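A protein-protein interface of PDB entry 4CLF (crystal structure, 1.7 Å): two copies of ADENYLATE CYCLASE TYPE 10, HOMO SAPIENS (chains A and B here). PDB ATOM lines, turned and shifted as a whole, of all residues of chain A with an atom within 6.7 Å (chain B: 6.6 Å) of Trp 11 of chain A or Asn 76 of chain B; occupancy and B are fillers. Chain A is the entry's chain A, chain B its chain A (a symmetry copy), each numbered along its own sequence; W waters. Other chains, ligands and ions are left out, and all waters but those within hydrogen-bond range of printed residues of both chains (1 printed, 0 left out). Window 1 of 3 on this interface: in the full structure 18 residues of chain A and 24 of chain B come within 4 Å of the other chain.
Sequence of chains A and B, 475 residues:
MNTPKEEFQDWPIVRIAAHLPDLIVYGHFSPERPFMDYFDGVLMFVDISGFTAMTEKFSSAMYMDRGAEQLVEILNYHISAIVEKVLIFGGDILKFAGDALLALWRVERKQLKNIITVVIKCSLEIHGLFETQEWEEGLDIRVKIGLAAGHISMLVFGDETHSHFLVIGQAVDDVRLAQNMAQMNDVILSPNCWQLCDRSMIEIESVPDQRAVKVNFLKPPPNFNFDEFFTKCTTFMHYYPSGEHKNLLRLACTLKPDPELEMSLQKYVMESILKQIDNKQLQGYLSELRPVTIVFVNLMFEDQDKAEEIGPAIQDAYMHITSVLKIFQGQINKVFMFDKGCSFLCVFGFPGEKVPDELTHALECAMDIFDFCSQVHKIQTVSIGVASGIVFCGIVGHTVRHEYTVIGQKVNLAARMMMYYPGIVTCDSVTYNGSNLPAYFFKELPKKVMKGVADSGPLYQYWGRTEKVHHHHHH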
ATOM      1  N   PHE A   8      16.802  33.078  15.064  1.00  0.00           N
ATOM      2  CA  PHE A   8      17.421  32.012  15.859  1.00  0.00           C
ATOM      3  C   PHE A   8      17.267  30.670  15.210  1.00  0.00           C
ATOM      4  O   PHE A   8      16.159  30.094  15.091  1.00  0.00           O
ATOM      5  CB  PHE A   8      16.986  31.979  17.341  1.00  0.00           C
ATOM      6  CG  PHE A   8      18.127  31.636  18.286  1.00  0.00           C
ATOM      7  CD1 PHE A   8      19.269  32.439  18.339  1.00  0.00           C
ATOM      8  CD2 PHE A   8      18.080  30.512  19.094  1.00  0.00           C
ATOM      9  CE1 PHE A   8      20.317  32.149  19.192  1.00  0.00           C
ATOM     10  CE2 PHE A   8      19.132  30.207  19.955  1.00  0.00           C
ATOM     11  CZ  PHE A   8      20.250  31.022  19.992  1.00  0.00           C
ATOM     12  N   GLN A   9      18.405  30.193  14.741  1.00  0.00           N
ATOM     13  CA  GLN A   9      18.478  28.785  14.485  1.00  0.00           C
ATOM     14  C   GLN A   9      19.639  28.237  15.331  1.00  0.00           C
ATOM     15  O   GLN A   9      20.379  27.419  14.771  1.00  0.00           O
ATOM     16  CB  GLN A   9      18.725  28.563  12.976  1.00  0.00           C
ATOM     17  CG  GLN A   9      17.648  29.151  12.037  1.00  0.00           C
ATOM     18  CD  GLN A   9      17.885  28.810  10.531  1.00  0.00           C
ATOM     19  OE1 GLN A   9      18.955  29.069   9.976  1.00  0.00           O
ATOM     20  NE2 GLN A   9      16.868  28.254   9.874  1.00  0.00           N
ATOM     21  N   ASP A  10      19.951  28.728  16.550  1.00  0.00           N
ATOM     22  CA  ASP A  10      21.198  28.119  17.200  1.00  0.00           C
ATOM     23  C   ASP A  10      20.875  27.410  18.492  1.00  0.00           C
ATOM     24  O   ASP A  10      21.674  27.345  19.427  1.00  0.00           O
ATOM     25  CB  ASP A  10      22.259  29.159  17.434  1.00  0.00           C
ATOM     26  CG  ASP A  10      23.611  28.592  17.715  1.00  0.00           C
ATOM     27  OD1 ASP A  10      23.976  27.456  17.328  1.00  0.00           O
ATOM     28  OD2 ASP A  10      24.338  29.421  18.329  1.00  0.00           O
ATOM     29  N   TRP A  11      19.732  26.800  18.487  1.00  0.00           N
ATOM     30  CA  TRP A  11      19.305  26.045  19.656  1.00  0.00           C
ATOM     31  C   TRP A  11      20.173  24.810  19.929  1.00  0.00           C
ATOM     32  O   TRP A  11      20.698  24.221  18.969  1.00  0.00           O
ATOM     33  CB  TRP A  11      17.883  25.564  19.359  1.00  0.00           C
ATOM     34  CG  TRP A  11      16.795  26.606  19.099  1.00  0.00           C
ATOM     35  CD1 TRP A  11      16.233  26.901  17.932  1.00  0.00           C
ATOM     36  CD2 TRP A  11      16.261  27.492  20.050  1.00  0.00           C
ATOM     37  NE1 TRP A  11      15.310  27.939  18.091  1.00  0.00           N
ATOM     38  CE2 TRP A  11      15.327  28.291  19.405  1.00  0.00           C
ATOM     39  CE3 TRP A  11      16.451  27.638  21.399  1.00  0.00           C
ATOM     40  CZ2 TRP A  11      14.587  29.255  20.077  1.00  0.00           C
ATOM     41  CZ3 TRP A  11      15.715  28.617  22.094  1.00  0.00           C
ATOM     42  CH2 TRP A  11      14.781  29.384  21.415  1.00  0.00           C
ATOM     43  N   PRO A  12      20.225  24.301  21.171  1.00  0.00           N
ATOM     44  CA  PRO A  12      20.850  23.060  21.444  1.00  0.00           C
ATOM     45  C   PRO A  12      20.482  21.911  20.507  1.00  0.00           C
ATOM     46  O   PRO A  12      21.368  21.181  20.089  1.00  0.00           O
ATOM     47  CB  PRO A  12      20.463  22.755  22.930  1.00  0.00           C
ATOM     48  CG  PRO A  12      20.331  24.129  23.522  1.00  0.00           C
ATOM     49  CD  PRO A  12      19.706  24.965  22.448  1.00  0.00           C
ATOM     50  N   ILE A  13      19.218  21.772  20.138  1.00  0.00           N
ATOM     51  CA  ILE A  13      18.827  20.629  19.280  1.00  0.00           C
ATOM     52  C   ILE A  13      19.538  20.746  17.916  1.00  0.00           C
ATOM     53  O   ILE A  13      19.923  19.723  17.341  1.00  0.00           O
ATOM     54  CB  ILE A  13      17.293  20.501  19.194  1.00  0.00           C
ATOM     55  CG1 ILE A  13      16.929  19.079  18.675  1.00  0.00           C
ATOM     56  CG2 ILE A  13      16.641  21.623  18.442  1.00  0.00           C
ATOM     57  CD1 ILE A  13      15.427  18.831  18.750  1.00  0.00           C
ATOM     58  N   VAL A  14      19.654  21.945  17.437  1.00  0.00           N
ATOM     59  CA  VAL A  14      20.334  22.179  16.133  1.00  0.00           C
ATOM     60  C   VAL A  14      21.839  21.809  16.237  1.00  0.00           C
ATOM     61  O   VAL A  14      22.454  21.185  15.377  1.00  0.00           O
ATOM     62  CB  VAL A  14      20.147  23.617  15.682  1.00  0.00           C
ATOM     63  CG1 VAL A  14      20.916  23.883  14.473  1.00  0.00           C
ATOM     64  CG2 VAL A  14      18.670  23.906  15.381  1.00  0.00           C
ATOM     65  N   ARG A  15      22.413  22.236  17.323  1.00  0.00           N
ATOM     66  CA  ARG A  15      23.855  21.995  17.580  1.00  0.00           C
ATOM     67  C   ARG A  15      24.075  20.512  17.694  1.00  0.00           C
ATOM     68  O   ARG A  15      25.071  20.002  17.194  1.00  0.00           O
ATOM     69  CB  ARG A  15      24.344  22.702  18.820  1.00  0.00           C
ATOM     70  CG  ARG A  15      24.279  24.214  18.747  1.00  0.00           C
ATOM     71  CD  ARG A  15      24.722  24.807  20.109  1.00  0.00           C
ATOM     72  NE  ARG A  15      25.076  26.205  19.876  1.00  0.00           N
ATOM     73  CZ  ARG A  15      25.844  26.932  20.715  1.00  0.00           C
ATOM     74  NH1 ARG A  15      26.375  26.367  21.820  1.00  0.00           N
ATOM     75  NH2 ARG A  15      26.139  28.207  20.382  1.00  0.00           N
ATOM     76  N   ILE A  16      23.196  19.767  18.364  1.00  0.00           N
ATOM     77  CA  ILE A  16      23.293  18.326  18.490  1.00  0.00           C
ATOM     78  C   ILE A  16      23.199  17.686  17.080  1.00  0.00           C
ATOM     79  O   ILE A  16      23.996  16.790  16.722  1.00  0.00           O
ATOM     80  CB  ILE A  16      22.258  17.784  19.453  1.00  0.00           C
ATOM     81  CG1 ILE A  16      22.600  18.217  20.883  1.00  0.00           C
ATOM     82  CG2 ILE A  16      22.150  16.250  19.315  1.00  0.00           C
ATOM     83  CD1 ILE A  16      21.495  18.025  21.885  1.00  0.00           C
ATOM     84  N   LEU A 255      15.770  22.730  12.562  1.00  0.00           N
ATOM     85  CA  LEU A 255      15.105  21.973  13.586  1.00  0.00           C
ATOM     86  C   LEU A 255      14.668  22.855  14.759  1.00  0.00           C
ATOM     87  O   LEU A 255      15.417  23.754  15.140  1.00  0.00           O
ATOM     88  CB  LEU A 255      16.031  20.890  14.110  1.00  0.00           C
ATOM     89  CG  LEU A 255      16.187  19.579  13.485  1.00  0.00           C
ATOM     90  CD1 LEU A 255      17.163  18.770  14.359  1.00  0.00           C
ATOM     91  CD2 LEU A 255      14.918  18.776  13.378  1.00  0.00           C
ATOM     92  N   LYS A 256      13.464  22.643  15.295  1.00  0.00           N
ATOM     93  CA  LYS A 256      13.080  23.476  16.428  1.00  0.00           C
ATOM     94  C   LYS A 256      13.111  22.610  17.677  1.00  0.00           C
ATOM     95  O   LYS A 256      12.998  21.389  17.612  1.00  0.00           O
ATOM     96  CB  LYS A 256      11.742  24.175  16.198  1.00  0.00           C
ATOM     97  CG  LYS A 256      11.739  25.040  14.916  1.00  0.00           C
ATOM     98  CD  LYS A 256      12.711  26.201  15.006  1.00  0.00           C
ATOM     99  CE  LYS A 256      12.750  26.961  13.667  1.00  0.00           C
ATOM    100  NZ  LYS A 256      13.992  27.733  13.600  1.00  0.00           N
ATOM    101  N   PRO A 257      13.190  23.260  18.831  1.00  0.00           N
ATOM    102  CA  PRO A 257      13.116  22.546  20.075  1.00  0.00           C
ATOM    103  C   PRO A 257      11.954  21.567  20.134  1.00  0.00           C
ATOM    104  O   PRO A 257      10.788  21.856  19.705  1.00  0.00           O
ATOM    105  CB  PRO A 257      13.014  23.665  21.068  1.00  0.00           C
ATOM    106  CG  PRO A 257      13.864  24.757  20.479  1.00  0.00           C
ATOM    107  CD  PRO A 257      13.428  24.698  19.050  1.00  0.00           C
ATOM    108  N   GLU A 262      15.105  15.644  21.135  1.00  0.00           N
ATOM    109  CA  GLU A 262      16.437  15.899  21.668  1.00  0.00           C
ATOM    110  C   GLU A 262      16.890  14.821  22.618  1.00  0.00           C
ATOM    111  O   GLU A 262      18.089  14.486  22.616  1.00  0.00           O
ATOM    112  CB  GLU A 262      16.431  17.282  22.369  1.00  0.00           C
ATOM    113  CG  GLU A 262      17.811  17.648  22.888  1.00  0.00           C
ATOM    114  CD  GLU A 262      17.970  19.135  23.283  1.00  0.00           C
ATOM    115  OE1 GLU A 262      17.374  20.005  22.599  1.00  0.00           O
ATOM    116  OE2 GLU A 262      18.684  19.409  24.292  1.00  0.00           O
ATOM    117  N   ILE A 277      28.106  22.180  23.817  1.00  0.00           N
ATOM    118  CA  ILE A 277      26.848  22.575  23.166  1.00  0.00           C
ATOM    119  C   ILE A 277      25.980  23.428  24.081  1.00  0.00           C
ATOM    120  O   ILE A 277      25.294  24.365  23.638  1.00  0.00           O
ATOM    121  CB  ILE A 277      26.119  21.330  22.635  1.00  0.00           C
ATOM    122  CG1 ILE A 277      26.804  20.815  21.348  1.00  0.00           C
ATOM    123  CG2 ILE A 277      24.617  21.560  22.430  1.00  0.00           C
ATOM    124  CD1 ILE A 277      26.280  19.514  20.867  1.00  0.00           C
ATOM    125  N   LEU B  71      14.878  22.321  29.523  1.00  0.00           N
ATOM    126  CA  LEU B  71      13.772  23.178  29.972  1.00  0.00           C
ATOM    127  C   LEU B  71      13.883  24.598  29.496  1.00  0.00           C
ATOM    128  O   LEU B  71      12.920  25.148  28.901  1.00  0.00           O
ATOM    129  CB  LEU B  71      13.632  23.137  31.518  1.00  0.00           C
ATOM    130  CG  LEU B  71      12.559  24.063  32.100  1.00  0.00           C
ATOM    131  CD1 LEU B  71      11.169  23.655  31.655  1.00  0.00           C
ATOM    132  CD2 LEU B  71      12.563  23.868  33.603  1.00  0.00           C
ATOM    133  N   VAL B  72      15.022  25.168  29.642  1.00  0.00           N
ATOM    134  CA  VAL B  72      15.265  26.550  29.234  1.00  0.00           C
ATOM    135  C   VAL B  72      15.087  26.680  27.706  1.00  0.00           C
ATOM    136  O   VAL B  72      14.526  27.633  27.234  1.00  0.00           O
ATOM    137  CB  VAL B  72      16.551  27.173  29.735  1.00  0.00           C
ATOM    138  CG1 VAL B  72      17.789  26.658  29.073  1.00  0.00           C
ATOM    139  CG2 VAL B  72      16.595  28.671  29.427  1.00  0.00           C
ATOM    140  N   GLU B  73      15.542  25.664  26.991  1.00  0.00           N
ATOM    141  CA  GLU B  73      15.400  25.659  25.529  1.00  0.00           C
ATOM    142  C   GLU B  73      13.926  25.701  25.092  1.00  0.00           C
ATOM    143  O   GLU B  73      13.542  26.528  24.267  1.00  0.00           O
ATOM    144  CB  GLU B  73      16.157  24.448  25.004  1.00  0.00           C
ATOM    145  CG  GLU B  73      16.015  24.341  23.483  1.00  0.00           C
ATOM    146  CD  GLU B  73      16.715  23.139  22.924  1.00  0.00           C
ATOM    147  OE1 GLU B  73      17.012  22.163  23.697  1.00  0.00           O
ATOM    148  OE2 GLU B  73      17.008  23.133  21.703  1.00  0.00           O
ATOM    149  N   ILE B  74      13.104  24.793  25.590  1.00  0.00           N
ATOM    150  CA  ILE B  74      11.711  24.700  25.174  1.00  0.00           C
ATOM    151  C   ILE B  74      10.912  25.915  25.694  1.00  0.00           C
ATOM    152  O   ILE B  74      10.082  26.498  24.996  1.00  0.00           O
ATOM    153  CB  ILE B  74      11.081  23.358  25.513  1.00  0.00           C
ATOM    154  CG1 ILE B  74       9.818  23.139  24.766  1.00  0.00           C
ATOM    155  CG2 ILE B  74      10.901  23.146  26.994  1.00  0.00           C
ATOM    156  CD1 ILE B  74       9.907  23.306  23.219  1.00  0.00           C
ATOM    157  N   LEU B  75      11.213  26.331  26.922  1.00  0.00           N
ATOM    158  CA  LEU B  75      10.530  27.510  27.476  1.00  0.00           C
ATOM    159  C   LEU B  75      10.867  28.764  26.656  1.00  0.00           C
ATOM    160  O   LEU B  75       9.931  29.497  26.205  1.00  0.00           O
ATOM    161  CB  LEU B  75      10.936  27.644  28.944  1.00  0.00           C
ATOM    162  CG  LEU B  75      10.180  28.738  29.638  1.00  0.00           C
ATOM    163  CD1 LEU B  75       8.716  28.354  29.694  1.00  0.00           C
ATOM    164  CD2 LEU B  75      10.809  28.932  31.013  1.00  0.00           C
ATOM    165  N   ASN B  76      12.148  28.951  26.338  1.00  0.00           N
ATOM    166  CA  ASN B  76      12.489  30.127  25.560  1.00  0.00           C
ATOM    167  C   ASN B  76      11.989  30.068  24.145  1.00  0.00           C
ATOM    168  O   ASN B  76      11.661  31.122  23.546  1.00  0.00           O
ATOM    169  CB  ASN B  76      13.989  30.398  25.612  1.00  0.00           C
ATOM    170  CG  ASN B  76      14.395  30.977  26.961  1.00  0.00           C
ATOM    171  OD1 ASN B  76      13.537  31.401  27.725  1.00  0.00           O
ATOM    172  ND2 ASN B  76      15.615  31.031  27.193  1.00  0.00           N
ATOM    173  N   TYR B  77      11.869  28.889  23.579  1.00  0.00           N
ATOM    174  CA  TYR B  77      11.288  28.774  22.219  1.00  0.00           C
ATOM    175  C   TYR B  77       9.877  29.370  22.201  1.00  0.00           C
ATOM    176  O   TYR B  77       9.537  30.228  21.315  1.00  0.00           O
ATOM    177  CB  TYR B  77      11.293  27.328  21.755  1.00  0.00           C
ATOM    178  CG  TYR B  77      10.634  27.093  20.455  1.00  0.00           C
ATOM    179  CD1 TYR B  77      11.133  27.686  19.314  1.00  0.00           C
ATOM    180  CD2 TYR B  77       9.597  26.248  20.362  1.00  0.00           C
ATOM    181  CE1 TYR B  77      10.554  27.442  18.092  1.00  0.00           C
ATOM    182  CE2 TYR B  77       9.031  25.960  19.152  1.00  0.00           C
ATOM    183  CZ  TYR B  77       9.506  26.585  18.028  1.00  0.00           C
ATOM    184  OH  TYR B  77       8.857  26.304  16.831  1.00  0.00           O
ATOM    185  N   HIS B  78       9.057  28.943  23.141  1.00  0.00           N
ATOM    186  CA  HIS B  78       7.667  29.412  23.198  1.00  0.00           C
ATOM    187  C   HIS B  78       7.571  30.829  23.705  1.00  0.00           C
ATOM    188  O   HIS B  78       6.762  31.609  23.153  1.00  0.00           O
ATOM    189  CB  HIS B  78       6.867  28.485  24.103  1.00  0.00           C
ATOM    190  CG  HIS B  78       6.654  27.127  23.479  1.00  0.00           C
ATOM    191  ND1 HIS B  78       6.188  26.967  22.195  1.00  0.00           N
ATOM    192  CD2 HIS B  78       6.973  25.895  23.920  1.00  0.00           C
ATOM    193  CE1 HIS B  78       6.134  25.670  21.912  1.00  0.00           C
ATOM    194  NE2 HIS B  78       6.588  25.001  22.949  1.00  0.00           N
ATOM    195  N   ILE B  79       8.293  31.134  24.779  1.00  0.00           N
ATOM    196  CA  ILE B  79       8.194  32.500  25.359  1.00  0.00           C
ATOM    197  C   ILE B  79       8.723  33.529  24.335  1.00  0.00           C
ATOM    198  O   ILE B  79       8.144  34.632  24.200  1.00  0.00           O
ATOM    199  CB  ILE B  79       8.881  32.624  26.683  1.00  0.00           C
ATOM    200  CG1 ILE B  79       8.136  31.744  27.692  1.00  0.00           C
ATOM    201  CG2 ILE B  79       8.947  34.090  27.131  1.00  0.00           C
ATOM    202  CD1 ILE B  79       8.856  31.640  28.976  1.00  0.00           C
ATOM    203  N   SER B  80       9.766  33.179  23.574  1.00  0.00           N
ATOM    204  CA  SER B  80      10.251  34.116  22.543  1.00  0.00           C
ATOM    205  C   SER B  80       9.182  34.535  21.562  1.00  0.00           C
ATOM    206  O   SER B  80       9.167  35.696  21.103  1.00  0.00           O
ATOM    207  CB  SER B  80      11.416  33.508  21.720  1.00  0.00           C
ATOM    208  OG  SER B  80      12.546  33.574  22.483  1.00  0.00           O
ATOM    209  N   ALA B  81       8.323  33.601  21.142  1.00  0.00           N
ATOM    210  CA  ALA B  81       7.283  33.868  20.196  1.00  0.00           C
ATOM    211  C   ALA B  81       6.286  34.871  20.773  1.00  0.00           C
ATOM    212  O   ALA B  81       5.762  35.757  20.073  1.00  0.00           O
ATOM    213  CB  ALA B  81       6.573  32.578  19.714  1.00  0.00           C
ATOM    214  N   ILE B 395      18.104  32.306  32.486  1.00  0.00           N
ATOM    215  CA  ILE B 395      17.653  33.496  31.771  1.00  0.00           C
ATOM    216  C   ILE B 395      16.549  33.074  30.812  1.00  0.00           C
ATOM    217  O   ILE B 395      16.807  32.296  29.851  1.00  0.00           O
ATOM    218  CB  ILE B 395      18.844  34.160  31.018  1.00  0.00           C
ATOM    219  CG1 ILE B 395      19.831  34.645  32.091  1.00  0.00           C
ATOM    220  CG2 ILE B 395      18.352  35.287  30.161  1.00  0.00           C
ATOM    221  CD1 ILE B 395      21.170  35.106  31.545  1.00  0.00           C
ATOM    222  N   VAL B 396      15.370  33.600  31.059  1.00  0.00           N
ATOM    223  CA  VAL B 396      14.189  33.241  30.311  1.00  0.00           C
ATOM    224  C   VAL B 396      13.690  34.418  29.473  1.00  0.00           C
ATOM    225  O   VAL B 396      13.646  35.542  29.929  1.00  0.00           O
ATOM    226  CB  VAL B 396      13.086  32.821  31.246  1.00  0.00           C
ATOM    227  CG1 VAL B 396      11.715  32.722  30.538  1.00  0.00           C
ATOM    228  CG2 VAL B 396      13.459  31.467  31.954  1.00  0.00           C
ATOM    229  N   GLY B 397      13.333  34.104  28.253  1.00  0.00           N
ATOM    230  CA  GLY B 397      12.800  35.126  27.351  1.00  0.00           C
ATOM    231  C   GLY B 397      13.457  35.071  26.007  1.00  0.00           C
ATOM    232  O   GLY B 397      13.873  34.006  25.506  1.00  0.00           O
ATOM    233  N   HIS B 398      13.371  36.171  25.287  1.00  0.00           N
ATOM    234  CA  HIS B 398      13.945  36.350  23.995  1.00  0.00           C
ATOM    235  C   HIS B 398      15.352  36.947  24.051  1.00  0.00           C
ATOM    236  O   HIS B 398      15.660  37.644  24.997  1.00  0.00           O
ATOM    237  CB  HIS B 398      13.072  37.374  23.188  1.00  0.00           C
ATOM    238  CG  HIS B 398      13.278  37.436  21.727  1.00  0.00           C
ATOM    239  ND1 HIS B 398      14.344  38.045  21.127  1.00  0.00           N
ATOM    240  CD2 HIS B 398      12.481  37.019  20.714  1.00  0.00           C
ATOM    241  CE1 HIS B 398      14.234  37.955  19.831  1.00  0.00           C
ATOM    242  NE2 HIS B 398      13.069  37.381  19.550  1.00  0.00           N
ATOM    243  N   HIS B 402      14.898  39.458  28.016  1.00  0.00           N
ATOM    244  CA  HIS B 402      14.933  38.287  28.848  1.00  0.00           C
ATOM    245  C   HIS B 402      15.343  38.636  30.254  1.00  0.00           C
ATOM    246  O   HIS B 402      15.885  39.719  30.490  1.00  0.00           O
ATOM    247  CB  HIS B 402      15.833  37.234  28.278  1.00  0.00           C
ATOM    248  CG  HIS B 402      17.230  37.681  27.956  1.00  0.00           C
ATOM    249  ND1 HIS B 402      17.960  37.036  26.996  1.00  0.00           N
ATOM    250  CD2 HIS B 402      18.055  38.663  28.432  1.00  0.00           C
ATOM    251  CE1 HIS B 402      19.134  37.627  26.845  1.00  0.00           C
ATOM    252  NE2 HIS B 402      19.243  38.577  27.742  1.00  0.00           N
HETATM  253  O   HOH W   1      14.570  20.514  22.236  1.00  0.00           O
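Among the printed residues, pairs that only touch across the chains: Trp 11 of chain A with Glu 73 of chain B (3.5 Å), Trp 11 of chain A with Tyr 77 of chain B (3.6 Å), Lys 256 of chain A with Tyr 77 of chain B (3.6 Å), Pro 257 of chain A with Glu 73 of chain B (3.7 Å), Pro 257 of chain A with Tyr 77 of chain B (3.8 Å), Pro 257 of chain A with Ile 74 of chain B (3.8 Å) and Trp 11 of chain A with Asn 76 of chain B (3.96 Å).
Of chain B, only Glu 73 (3.5 Å), Asn 76 (3.96 Å) and Tyr 77 (3.6 Å) come within 4 Å of Trp 11 of chain A. Of the printed residues of chain B, Pro 12 of chain A touches Glu 73. Of the printed residues of chain B, Pro 257 of chain A touches Glu 73 (3.7 Å), Ile 74 (3.8 Å) and Tyr 77 (3.8 Å). Of the printed residues of chain B, Glu 262 of chain A touches Glu 73 (2.4 Å). The nearest printed residue of chain B that does not touch Glu 262 of chain A is Ile 74 of chain B (7.1 Å).
No position is printed for both chains. Of the 10 pairs that touch across the chains among the printed residues, none has its exchanged pair printed and touching as well.
Water W1 bridges the side-chain carboxylate of Glu 262 of chain A (2.9 Å) and the side-chain carboxylate of Glu 73 of chain B (3.3 Å).
Along chain A the printed residues that touch a printed residue of chain B span positions 11 to 262. Among the printed residues, 10 pairs touch across the chains. Among the printed residues, no Asp or Glu carboxylate lies within 4 Å of a Lys or Arg side-chain nitrogen of the other chain.
OE1 of Glu 73 of chain B sits close to OE1 of Glu 262 of chain A (2.4 Å). The backbone NH (N) of Ile 13 of chain A lies within hydrogen-bond range of the side-chain carboxylate (OE2) of Glu 73 of chain B (3.0 Å). N of Pro 12 of chain A sits close to OE2 of Glu 73 of chain B, 3.5 Å away.
The backbone NH of Gly 397 of chain B sits at hydrogen-bond distance from the side-chain amide oxygen of Asn 76 of chain B (2.8 Å). The backbone carbonyl oxygen of Asn 76 of chain B sits at hydrogen-bond distance from the side-chain hydroxyl of Ser 80 of chain B (2.8 Å). The backbone carbonyl oxygen (O) of Ile 395 of chain B lies within hydrogen-bond range of the side-chain amide nitrogen (ND2) of Asn 76 of chain B, at 3.2 Å.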
